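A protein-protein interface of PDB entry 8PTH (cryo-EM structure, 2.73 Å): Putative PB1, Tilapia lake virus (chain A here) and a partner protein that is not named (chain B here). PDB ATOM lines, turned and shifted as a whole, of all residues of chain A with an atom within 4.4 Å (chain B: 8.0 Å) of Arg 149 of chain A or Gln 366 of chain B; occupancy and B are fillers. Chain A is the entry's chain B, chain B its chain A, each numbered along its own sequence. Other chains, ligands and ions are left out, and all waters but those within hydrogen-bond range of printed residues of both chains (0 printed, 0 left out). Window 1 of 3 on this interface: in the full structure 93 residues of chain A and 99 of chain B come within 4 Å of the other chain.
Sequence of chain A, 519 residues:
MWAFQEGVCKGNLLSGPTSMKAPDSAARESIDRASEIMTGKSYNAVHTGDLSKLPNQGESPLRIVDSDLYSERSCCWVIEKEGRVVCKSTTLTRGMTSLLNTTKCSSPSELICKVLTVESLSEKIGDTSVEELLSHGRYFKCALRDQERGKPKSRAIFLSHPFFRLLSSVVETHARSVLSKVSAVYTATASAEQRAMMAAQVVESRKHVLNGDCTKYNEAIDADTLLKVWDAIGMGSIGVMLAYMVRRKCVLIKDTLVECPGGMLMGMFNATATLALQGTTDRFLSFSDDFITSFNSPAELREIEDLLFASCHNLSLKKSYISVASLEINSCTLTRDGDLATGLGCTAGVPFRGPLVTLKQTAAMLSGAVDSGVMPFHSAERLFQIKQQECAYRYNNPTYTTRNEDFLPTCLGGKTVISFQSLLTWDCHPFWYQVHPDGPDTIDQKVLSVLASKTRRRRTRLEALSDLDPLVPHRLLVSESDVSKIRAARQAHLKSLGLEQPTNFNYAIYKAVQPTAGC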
ATOM      1  N   LYS A  10      21.645   4.169  -6.718  1.00  0.00           N
ATOM      2  CA  LYS A  10      21.428   2.957  -7.494  1.00  0.00           C
ATOM      3  C   LYS A  10      21.866   1.695  -6.762  1.00  0.00           C
ATOM      4  O   LYS A  10      21.717   0.598  -7.310  1.00  0.00           O
ATOM      5  CB  LYS A  10      22.171   3.052  -8.829  1.00  0.00           C
ATOM      6  CG  LYS A  10      21.348   3.669  -9.945  1.00  0.00           C
ATOM      7  CD  LYS A  10      22.215   4.425 -10.940  1.00  0.00           C
ATOM      8  CE  LYS A  10      21.417   5.490 -11.673  1.00  0.00           C
ATOM      9  NZ  LYS A  10      21.746   6.862 -11.195  1.00  0.00           N
ATOM     10  N   ASN A  12      25.014   0.724  -5.942  1.00  0.00           N
ATOM     11  CA  ASN A  12      26.189   0.182  -6.609  1.00  0.00           C
ATOM     12  C   ASN A  12      27.361  -0.040  -5.661  1.00  0.00           C
ATOM     13  O   ASN A  12      28.462  -0.352  -6.123  1.00  0.00           O
ATOM     14  CB  ASN A  12      26.626   1.116  -7.742  1.00  0.00           C
ATOM     15  CG  ASN A  12      25.807   0.932  -9.001  1.00  0.00           C
ATOM     16  OD1 ASN A  12      25.000   0.010  -9.104  1.00  0.00           O
ATOM     17  ND2 ASN A  12      26.013   1.813  -9.970  1.00  0.00           N
ATOM     18  N   LEU A  14      28.101  -2.389  -3.470  1.00  0.00           N
ATOM     19  CA  LEU A  14      28.624  -3.745  -3.469  1.00  0.00           C
ATOM     20  C   LEU A  14      28.983  -4.180  -4.888  1.00  0.00           C
ATOM     21  O   LEU A  14      28.587  -3.564  -5.879  1.00  0.00           O
ATOM     22  CB  LEU A  14      27.611  -4.712  -2.857  1.00  0.00           C
ATOM     23  CG  LEU A  14      27.252  -4.494  -1.385  1.00  0.00           C
ATOM     24  CD1 LEU A  14      26.279  -5.563  -0.919  1.00  0.00           C
ATOM     25  CD2 LEU A  14      28.495  -4.488  -0.511  1.00  0.00           C
ATOM     26  N   SER A  15      29.750  -5.263  -4.975  1.00  0.00           N
ATOM     27  CA  SER A  15      30.165  -5.785  -6.266  1.00  0.00           C
ATOM     28  C   SER A  15      28.976  -6.383  -7.013  1.00  0.00           C
ATOM     29  O   SER A  15      27.920  -6.663  -6.439  1.00  0.00           O
ATOM     30  CB  SER A  15      31.252  -6.845  -6.091  1.00  0.00           C
ATOM     31  OG  SER A  15      32.356  -6.330  -5.371  1.00  0.00           O
ATOM     32  N   GLY A  16      29.161  -6.575  -8.314  1.00  0.00           N
ATOM     33  CA  GLY A  16      28.142  -7.161  -9.148  1.00  0.00           C
ATOM     34  C   GLY A  16      27.995  -8.647  -8.893  1.00  0.00           C
ATOM     35  O   GLY A  16      28.813  -9.265  -8.206  1.00  0.00           O
ATOM     36  N   PRO A  17      26.946  -9.250  -9.443  1.00  0.00           N
ATOM     37  CA  PRO A  17      26.711 -10.678  -9.212  1.00  0.00           C
ATOM     38  C   PRO A  17      27.785 -11.545  -9.851  1.00  0.00           C
ATOM     39  O   PRO A  17      28.532 -11.118 -10.733  1.00  0.00           O
ATOM     40  CB  PRO A  17      25.343 -10.925  -9.858  1.00  0.00           C
ATOM     41  CG  PRO A  17      25.180  -9.822 -10.844  1.00  0.00           C
ATOM     42  CD  PRO A  17      25.895  -8.641 -10.274  1.00  0.00           C
ATOM     43  N   GLU A 148      27.125  -7.923 -14.516  1.00  0.00           N
ATOM     44  CA  GLU A 148      26.856  -6.507 -14.321  1.00  0.00           C
ATOM     45  C   GLU A 148      25.880  -6.325 -13.169  1.00  0.00           C
ATOM     46  O   GLU A 148      25.037  -7.187 -12.907  1.00  0.00           O
ATOM     47  CB  GLU A 148      26.296  -5.869 -15.598  1.00  0.00           C
ATOM     48  CG  GLU A 148      25.095  -6.602 -16.181  1.00  0.00           C
ATOM     49  CD  GLU A 148      25.467  -7.540 -17.318  1.00  0.00           C
ATOM     50  OE1 GLU A 148      26.595  -7.437 -17.843  1.00  0.00           O
ATOM     51  OE2 GLU A 148      24.629  -8.393 -17.685  1.00  0.00           O
ATOM     52  N   ARG A 149      26.002  -5.190 -12.481  1.00  0.00           N
ATOM     53  CA  ARG A 149      25.133  -4.911 -11.347  1.00  0.00           C
ATOM     54  C   ARG A 149      23.678  -4.827 -11.793  1.00  0.00           C
ATOM     55  O   ARG A 149      23.367  -4.289 -12.858  1.00  0.00           O
ATOM     56  CB  ARG A 149      25.546  -3.603 -10.671  1.00  0.00           C
ATOM     57  CG  ARG A 149      26.950  -3.612 -10.093  1.00  0.00           C
ATOM     58  CD  ARG A 149      27.081  -2.636  -8.937  1.00  0.00           C
ATOM     59  NE  ARG A 149      28.418  -2.643  -8.359  1.00  0.00           N
ATOM     60  CZ  ARG A 149      29.485  -2.097  -8.927  1.00  0.00           C
ATOM     61  NH1 ARG A 149      29.408  -1.489 -10.099  1.00  0.00           N
ATOM     62  NH2 ARG A 149      30.657  -2.164  -8.305  1.00  0.00           N
ATOM     63  N   GLY A 150      22.785  -5.362 -10.965  1.00  0.00           N
ATOM     64  CA  GLY A 150      21.365  -5.288 -11.234  1.00  0.00           C
ATOM     65  C   GLY A 150      20.825  -6.346 -12.167  1.00  0.00           C
ATOM     66  O   GLY A 150      19.646  -6.280 -12.529  1.00  0.00           O
ATOM     67  N   LYS A 151      21.642  -7.318 -12.568  1.00  0.00           N
ATOM     68  CA  LYS A 151      21.224  -8.396 -13.461  1.00  0.00           C
ATOM     69  C   LYS A 151      21.583  -9.720 -12.803  1.00  0.00           C
ATOM     70  O   LYS A 151      22.586 -10.354 -13.158  1.00  0.00           O
ATOM     71  CB  LYS A 151      21.882  -8.267 -14.836  1.00  0.00           C
ATOM     72  CG  LYS A 151      21.521  -6.992 -15.580  1.00  0.00           C
ATOM     73  CD  LYS A 151      20.153  -7.097 -16.230  1.00  0.00           C
ATOM     74  CE  LYS A 151      19.515  -5.729 -16.408  1.00  0.00           C
ATOM     75  NZ  LYS A 151      20.452  -4.744 -17.014  1.00  0.00           N
ATOM     76  N   ALA A 348      30.333   3.619  -6.703  1.00  0.00           N
ATOM     77  CA  ALA A 348      30.570   2.194  -6.536  1.00  0.00           C
ATOM     78  C   ALA A 348      31.657   1.976  -5.495  1.00  0.00           C
ATOM     79  O   ALA A 348      32.641   2.721  -5.444  1.00  0.00           O
ATOM     80  CB  ALA A 348      30.978   1.544  -7.860  1.00  0.00           C
ATOM     81  N   GLN B 311      34.036  -8.146   0.120  1.00  0.00           N
ATOM     82  CA  GLN B 311      33.179  -7.006   0.407  1.00  0.00           C
ATOM     83  C   GLN B 311      33.679  -6.245   1.628  1.00  0.00           C
ATOM     84  O   GLN B 311      34.174  -6.839   2.589  1.00  0.00           O
ATOM     85  CB  GLN B 311      31.738  -7.465   0.633  1.00  0.00           C
ATOM     86  CG  GLN B 311      31.108  -8.169  -0.562  1.00  0.00           C
ATOM     87  CD  GLN B 311      31.414  -7.483  -1.880  1.00  0.00           C
ATOM     88  OE1 GLN B 311      31.135  -6.299  -2.054  1.00  0.00           O
ATOM     89  NE2 GLN B 311      31.992  -8.228  -2.813  1.00  0.00           N
ATOM     90  N   THR B 358      24.044 -13.166  -5.710  1.00  0.00           N
ATOM     91  CA  THR B 358      23.306 -12.717  -6.882  1.00  0.00           C
ATOM     92  C   THR B 358      22.973 -11.234  -6.834  1.00  0.00           C
ATOM     93  O   THR B 358      22.666 -10.647  -7.878  1.00  0.00           O
ATOM     94  CB  THR B 358      22.008 -13.516  -7.034  1.00  0.00           C
ATOM     95  OG1 THR B 358      21.114 -13.196  -5.962  1.00  0.00           O
ATOM     96  CG2 THR B 358      22.293 -15.009  -7.024  1.00  0.00           C
ATOM     97  N   ARG B 359      23.025 -10.619  -5.654  1.00  0.00           N
ATOM     98  CA  ARG B 359      22.836  -9.180  -5.502  1.00  0.00           C
ATOM     99  C   ARG B 359      21.534  -8.720  -6.156  1.00  0.00           C
ATOM    100  O   ARG B 359      21.491  -7.736  -6.895  1.00  0.00           O
ATOM    101  CB  ARG B 359      24.033  -8.416  -6.071  1.00  0.00           C
ATOM    102  CG  ARG B 359      25.386  -8.876  -5.539  1.00  0.00           C
ATOM    103  CD  ARG B 359      25.767  -8.147  -4.263  1.00  0.00           C
ATOM    104  NE  ARG B 359      26.503  -9.005  -3.341  1.00  0.00           N
ATOM    105  CZ  ARG B 359      27.800  -9.266  -3.429  1.00  0.00           C
ATOM    106  NH1 ARG B 359      28.549  -8.746  -4.388  1.00  0.00           N
ATOM    107  NH2 ARG B 359      28.362 -10.069  -2.531  1.00  0.00           N
ATOM    108  N   VAL B 360      20.454  -9.456  -5.880  1.00  0.00           N
ATOM    109  CA  VAL B 360      19.138  -9.047  -6.362  1.00  0.00           C
ATOM    110  C   VAL B 360      18.731  -7.722  -5.733  1.00  0.00           C
ATOM    111  O   VAL B 360      17.926  -6.967  -6.301  1.00  0.00           O
ATOM    112  CB  VAL B 360      18.107 -10.158  -6.076  1.00  0.00           C
ATOM    113  CG1 VAL B 360      17.847 -10.279  -4.582  1.00  0.00           C
ATOM    114  CG2 VAL B 360      16.815  -9.896  -6.831  1.00  0.00           C
ATOM    115  N   SER B 361      19.276  -7.417  -4.554  1.00  0.00           N
ATOM    116  CA  SER B 361      19.021  -6.125  -3.935  1.00  0.00           C
ATOM    117  C   SER B 361      19.445  -4.982  -4.846  1.00  0.00           C
ATOM    118  O   SER B 361      18.853  -3.903  -4.795  1.00  0.00           O
ATOM    119  CB  SER B 361      19.746  -6.033  -2.593  1.00  0.00           C
ATOM    120  OG  SER B 361      21.095  -5.641  -2.764  1.00  0.00           O
ATOM    121  N   GLN B 362      20.458  -5.196  -5.689  1.00  0.00           N
ATOM    122  CA  GLN B 362      20.853  -4.161  -6.639  1.00  0.00           C
ATOM    123  C   GLN B 362      19.745  -3.892  -7.651  1.00  0.00           C
ATOM    124  O   GLN B 362      19.452  -2.733  -7.971  1.00  0.00           O
ATOM    125  CB  GLN B 362      22.142  -4.567  -7.350  1.00  0.00           C
ATOM    126  CG  GLN B 362      23.397  -3.981  -6.732  1.00  0.00           C
ATOM    127  CD  GLN B 362      24.619  -4.847  -6.953  1.00  0.00           C
ATOM    128  OE1 GLN B 362      24.590  -5.795  -7.735  1.00  0.00           O
ATOM    129  NE2 GLN B 362      25.705  -4.522  -6.263  1.00  0.00           N
ATOM    130  N   ALA B 363      19.119  -4.950  -8.168  1.00  0.00           N
ATOM    131  CA  ALA B 363      18.000  -4.767  -9.086  1.00  0.00           C
ATOM    132  C   ALA B 363      16.840  -4.063  -8.396  1.00  0.00           C
ATOM    133  O   ALA B 363      16.216  -3.159  -8.970  1.00  0.00           O
ATOM    134  CB  ALA B 363      17.552  -6.118  -9.641  1.00  0.00           C
ATOM    135  N   VAL B 364      16.539  -4.461  -7.158  1.00  0.00           N
ATOM    136  CA  VAL B 364      15.457  -3.809  -6.428  1.00  0.00           C
ATOM    137  C   VAL B 364      15.776  -2.333  -6.218  1.00  0.00           C
ATOM    138  O   VAL B 364      14.899  -1.472  -6.335  1.00  0.00           O
ATOM    139  CB  VAL B 364      15.196  -4.528  -5.092  1.00  0.00           C
ATOM    140  CG1 VAL B 364      14.076  -3.838  -4.330  1.00  0.00           C
ATOM    141  CG2 VAL B 364      14.846  -5.984  -5.332  1.00  0.00           C
ATOM    142  N   ALA B 365      17.034  -2.020  -5.899  1.00  0.00           N
ATOM    143  CA  ALA B 365      17.428  -0.632  -5.682  1.00  0.00           C
ATOM    144  C   ALA B 365      17.310   0.186  -6.960  1.00  0.00           C
ATOM    145  O   ALA B 365      16.868   1.339  -6.924  1.00  0.00           O
ATOM    146  CB  ALA B 365      18.857  -0.573  -5.145  1.00  0.00           C
ATOM    147  N   GLN B 366      17.715  -0.381  -8.097  1.00  0.00           N
ATOM    148  CA  GLN B 366      17.580   0.341  -9.359  1.00  0.00           C
ATOM    149  C   GLN B 366      16.115   0.612  -9.679  1.00  0.00           C
ATOM    150  O   GLN B 366      15.748   1.727 -10.085  1.00  0.00           O
ATOM    151  CB  GLN B 366      18.238  -0.451 -10.486  1.00  0.00           C
ATOM    152  CG  GLN B 366      19.754  -0.433 -10.438  1.00  0.00           C
ATOM    153  CD  GLN B 366      20.380  -1.395 -11.426  1.00  0.00           C
ATOM    154  OE1 GLN B 366      19.721  -1.871 -12.348  1.00  0.00           O
ATOM    155  NE2 GLN B 366      21.661  -1.684 -11.236  1.00  0.00           N
ATOM    156  N   HIS B 367      15.256  -0.391  -9.486  1.00  0.00           N
ATOM    157  CA  HIS B 367      13.839  -0.180  -9.752  1.00  0.00           C
ATOM    158  C   HIS B 367      13.245   0.845  -8.795  1.00  0.00           C
ATOM    159  O   HIS B 367      12.395   1.648  -9.188  1.00  0.00           O
ATOM    160  CB  HIS B 367      13.076  -1.499  -9.668  1.00  0.00           C
ATOM    161  CG  HIS B 367      11.797  -1.495 -10.443  1.00  0.00           C
ATOM    162  ND1 HIS B 367      11.744  -1.184 -11.785  1.00  0.00           N
ATOM    163  CD2 HIS B 367      10.522  -1.748 -10.065  1.00  0.00           C
ATOM    164  CE1 HIS B 367      10.493  -1.252 -12.201  1.00  0.00           C
ATOM    165  NE2 HIS B 367       9.731  -1.593 -11.177  1.00  0.00           N
ATOM    166  N   PHE B 368      13.679   0.837  -7.533  1.00  0.00           N
ATOM    167  CA  PHE B 368      13.170   1.814  -6.577  1.00  0.00           C
ATOM    168  C   PHE B 368      13.654   3.219  -6.912  1.00  0.00           C
ATOM    169  O   PHE B 368      12.938   4.198  -6.684  1.00  0.00           O
ATOM    170  CB  PHE B 368      13.585   1.431  -5.158  1.00  0.00           C
ATOM    171  CG  PHE B 368      12.956   2.281  -4.093  1.00  0.00           C
ATOM    172  CD1 PHE B 368      11.581   2.411  -4.014  1.00  0.00           C
ATOM    173  CD2 PHE B 368      13.740   2.952  -3.173  1.00  0.00           C
ATOM    174  CE1 PHE B 368      11.001   3.193  -3.038  1.00  0.00           C
ATOM    175  CE2 PHE B 368      13.163   3.736  -2.195  1.00  0.00           C
ATOM    176  CZ  PHE B 368      11.793   3.855  -2.127  1.00  0.00           C
ATOM    177  N   ASN B 369      14.873   3.341  -7.439  1.00  0.00           N
ATOM    178  CA  ASN B 369      15.339   4.639  -7.914  1.00  0.00           C
ATOM    179  C   ASN B 369      14.455   5.145  -9.046  1.00  0.00           C
ATOM    180  O   ASN B 369      14.030   6.308  -9.047  1.00  0.00           O
ATOM    181  CB  ASN B 369      16.793   4.535  -8.370  1.00  0.00           C
ATOM    182  CG  ASN B 369      17.442   5.887  -8.567  1.00  0.00           C
ATOM    183  OD1 ASN B 369      17.438   6.727  -7.668  1.00  0.00           O
ATOM    184  ND2 ASN B 369      18.004   6.106  -9.748  1.00  0.00           N
ATOM    185  N   ARG B 370      14.149   4.274 -10.011  1.00  0.00           N
ATOM    186  CA  ARG B 370      13.216   4.657 -11.067  1.00  0.00           C
ATOM    187  C   ARG B 370      11.868   5.066 -10.482  1.00  0.00           C
ATOM    188  O   ARG B 370      11.269   6.057 -10.910  1.00  0.00           O
ATOM    189  CB  ARG B 370      13.038   3.509 -12.059  1.00  0.00           C
ATOM    190  CG  ARG B 370      14.181   3.351 -13.042  1.00  0.00           C
ATOM    191  CD  ARG B 370      13.823   2.377 -14.148  1.00  0.00           C
ATOM    192  NE  ARG B 370      13.817   0.995 -13.681  1.00  0.00           N
ATOM    193  CZ  ARG B 370      14.878   0.200 -13.663  1.00  0.00           C
ATOM    194  NH1 ARG B 370      16.063   0.616 -14.079  1.00  0.00           N
ATOM    195  NH2 ARG B 370      14.747  -1.043 -13.215  1.00  0.00           N
ATOM    196  N   HIS B 371      11.383   4.309  -9.496  1.00  0.00           N
ATOM    197  CA  HIS B 371      10.099   4.611  -8.870  1.00  0.00           C
ATOM    198  C   HIS B 371      10.114   5.989  -8.223  1.00  0.00           C
ATOM    199  O   HIS B 371       9.154   6.758  -8.355  1.00  0.00           O
ATOM    200  CB  HIS B 371       9.781   3.529  -7.835  1.00  0.00           C
ATOM    201  CG  HIS B 371       8.458   3.698  -7.152  1.00  0.00           C
ATOM    202  ND1 HIS B 371       8.027   2.844  -6.159  1.00  0.00           N
ATOM    203  CD2 HIS B 371       7.470   4.607  -7.319  1.00  0.00           C
ATOM    204  CE1 HIS B 371       6.835   3.225  -5.740  1.00  0.00           C
ATOM    205  NE2 HIS B 371       6.473   4.293  -6.429  1.00  0.00           N
ATOM    206  N   ARG B 372      11.194   6.318  -7.517  1.00  0.00           N
ATOM    207  CA  ARG B 372      11.287   7.605  -6.842  1.00  0.00           C
ATOM    208  C   ARG B 372      11.476   8.757  -7.816  1.00  0.00           C
ATOM    209  O   ARG B 372      11.118   9.892  -7.489  1.00  0.00           O
ATOM    210  CB  ARG B 372      12.438   7.589  -5.838  1.00  0.00           C
ATOM    211  CG  ARG B 372      12.080   6.977  -4.496  1.00  0.00           C
ATOM    212  CD  ARG B 372      12.920   7.565  -3.380  1.00  0.00           C
ATOM    213  NE  ARG B 372      14.315   7.154  -3.476  1.00  0.00           N
ATOM    214  CZ  ARG B 372      15.352   7.910  -3.141  1.00  0.00           C
ATOM    215  NH1 ARG B 372      15.194   9.138  -2.675  1.00  0.00           N
ATOM    216  NH2 ARG B 372      16.581   7.420  -3.276  1.00  0.00           N
ATOM    217  N   LEU B 373      12.031   8.497  -9.000  1.00  0.00           N
ATOM    218  CA  LEU B 373      12.230   9.541  -9.994  1.00  0.00           C
ATOM    219  C   LEU B 373      11.072   9.677 -10.975  1.00  0.00           C
ATOM    220  O   LEU B 373      11.112  10.569 -11.828  1.00  0.00           O
ATOM    221  CB  LEU B 373      13.517   9.277 -10.783  1.00  0.00           C
ATOM    222  CG  LEU B 373      14.825   9.556 -10.045  1.00  0.00           C
ATOM    223  CD1 LEU B 373      15.990   8.931 -10.788  1.00  0.00           C
ATOM    224  CD2 LEU B 373      15.035  11.050  -9.871  1.00  0.00           C
ATOM    225  N   PHE B 382       4.983  -1.511 -14.771  1.00  0.00           N
ATOM    226  CA  PHE B 382       6.045  -1.058 -13.882  1.00  0.00           C
ATOM    227  C   PHE B 382       6.016  -1.824 -12.568  1.00  0.00           C
ATOM    228  O   PHE B 382       7.065  -2.216 -12.045  1.00  0.00           O
ATOM    229  CB  PHE B 382       5.908   0.443 -13.634  1.00  0.00           C
ATOM    230  CG  PHE B 382       7.017   1.028 -12.810  1.00  0.00           C
ATOM    231  CD1 PHE B 382       6.937   1.047 -11.428  1.00  0.00           C
ATOM    232  CD2 PHE B 382       8.138   1.565 -13.417  1.00  0.00           C
ATOM    233  CE1 PHE B 382       7.955   1.588 -10.671  1.00  0.00           C
ATOM    234  CE2 PHE B 382       9.158   2.108 -12.663  1.00  0.00           C
ATOM    235  CZ  PHE B 382       9.067   2.119 -11.289  1.00  0.00           C
ATOM    236  N   GLY B 385       8.128  -5.135 -11.783  1.00  0.00           N
ATOM    237  CA  GLY B 385       9.568  -4.990 -11.832  1.00  0.00           C
ATOM    238  C   GLY B 385      10.176  -5.357 -10.497  1.00  0.00           C
ATOM    239  O   GLY B 385      11.375  -5.632 -10.397  1.00  0.00           O
ATOM    240  N   TYR B 386       9.343  -5.355  -9.456  1.00  0.00           N
ATOM    241  CA  TYR B 386       9.729  -5.838  -8.141  1.00  0.00           C
ATOM    242  C   TYR B 386       9.534  -7.339  -7.988  1.00  0.00           C
ATOM    243  O   TYR B 386       9.966  -7.905  -6.979  1.00  0.00           O
ATOM    244  CB  TYR B 386       8.919  -5.113  -7.061  1.00  0.00           C
ATOM    245  CG  TYR B 386       9.224  -3.637  -6.946  1.00  0.00           C
ATOM    246  CD1 TYR B 386      10.461  -3.197  -6.497  1.00  0.00           C
ATOM    247  CD2 TYR B 386       8.275  -2.685  -7.283  1.00  0.00           C
ATOM    248  CE1 TYR B 386      10.743  -1.852  -6.388  1.00  0.00           C
ATOM    249  CE2 TYR B 386       8.547  -1.337  -7.179  1.00  0.00           C
ATOM    250  CZ  TYR B 386       9.782  -0.925  -6.730  1.00  0.00           C
ATOM    251  OH  TYR B 386      10.059   0.416  -6.623  1.00  0.00           O
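Hydrophobic or aromatic side chains of chain A within 4 Å of the printed part of chain B: Leu 14 and Pro 17. Of the 20 printed residues of chain B, 8 touch a printed residue of chain A. Among the printed residues, 15 pairs touch across the chains. Among the printed residues, no Asp or Glu carboxylate lies within 4 Å of a Lys or Arg side-chain nitrogen of the other chain.
Lys 10 of chain A touches Ala 365 of chain B. Lys 10 of chain A touches Gln 366 of chain B. ND2 of Asn 369 of chain B touches CE of Lys 10 of chain A, at 3.97 Å. Gly 16 of chain A touches Arg 359 of chain B (O to NH1, 3.9 Å). Thr 358 of chain B touches Pro 17 of chain A (O to CB, 3.3 Å). Arg 149 of chain A touches Gln 362 of chain B. Arg 149 of chain A touches Gln 366 of chain B (O to NE2, 3.5 Å). Gln 362 of chain B touches Gly 150 of chain A (OE1 to N, 3.7 Å). Ala 363 of chain B touches Gly 150 of chain A (CB to O, 3.6 Å). Gly 150 of chain A touches Gln 366 of chain B (CA to NE2, 3.6 Å).
The backbone carbonyl oxygen (O) of Leu 14 of chain A lies within hydrogen-bond range of the side-chain amide nitrogen (NE2) of Gln 362 of chain B. NE2 of Gln 362 of chain B sits at hydrogen-bond distance from O of Ser 15 of chain A. The backbone carbonyl oxygen (O) of Ser 15 of chain A is in hydrogen-bond range of the guanidinium group (NH1) of Arg 359 of chain B. The side-chain amide nitrogen of Gln 311 of chain B sits at hydrogen-bond distance from the side-chain hydroxyl of Ser 15 of chain A, 3.2 Å away.
The guanidinium group (NE) of Arg 149 of chain A sits at hydrogen-bond distance from the backbone carbonyl oxygen (O) of Asn 12 of chain A (3.2 Å). The backbone carbonyl oxygen of Leu 14 of chain A is in hydrogen-bond range of the guanidinium group of Arg 149 of chain A (2.7 Å).
Of the printed residues of chain A, Gln 311 of chain B touches Leu 14 and Ser 15. Printed residues of chain A within 4 Å of Ala 363 of chain B: Gly 150 (3.6 Å). Of the printed residues of chain A, Ala 365 of chain B touches Lys 10. Gln 366 of chain B touches just these residues of chain A: Lys 10, Arg 149 and Gly 150. Printed residues of chain A within 4 Å of Asn 369 of chain B: Lys 10 (3.97 Å). Phe 382 of chain B touches none of the printed residues of chain A. The nearest residue of chain B that does not touch Arg 149 of chain A is Ala 363 of chain B (5.8 Å). The nearest printed residue of chain B that does not touch Gly 150 of chain A is Arg 359 of chain B (4.9 Å).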
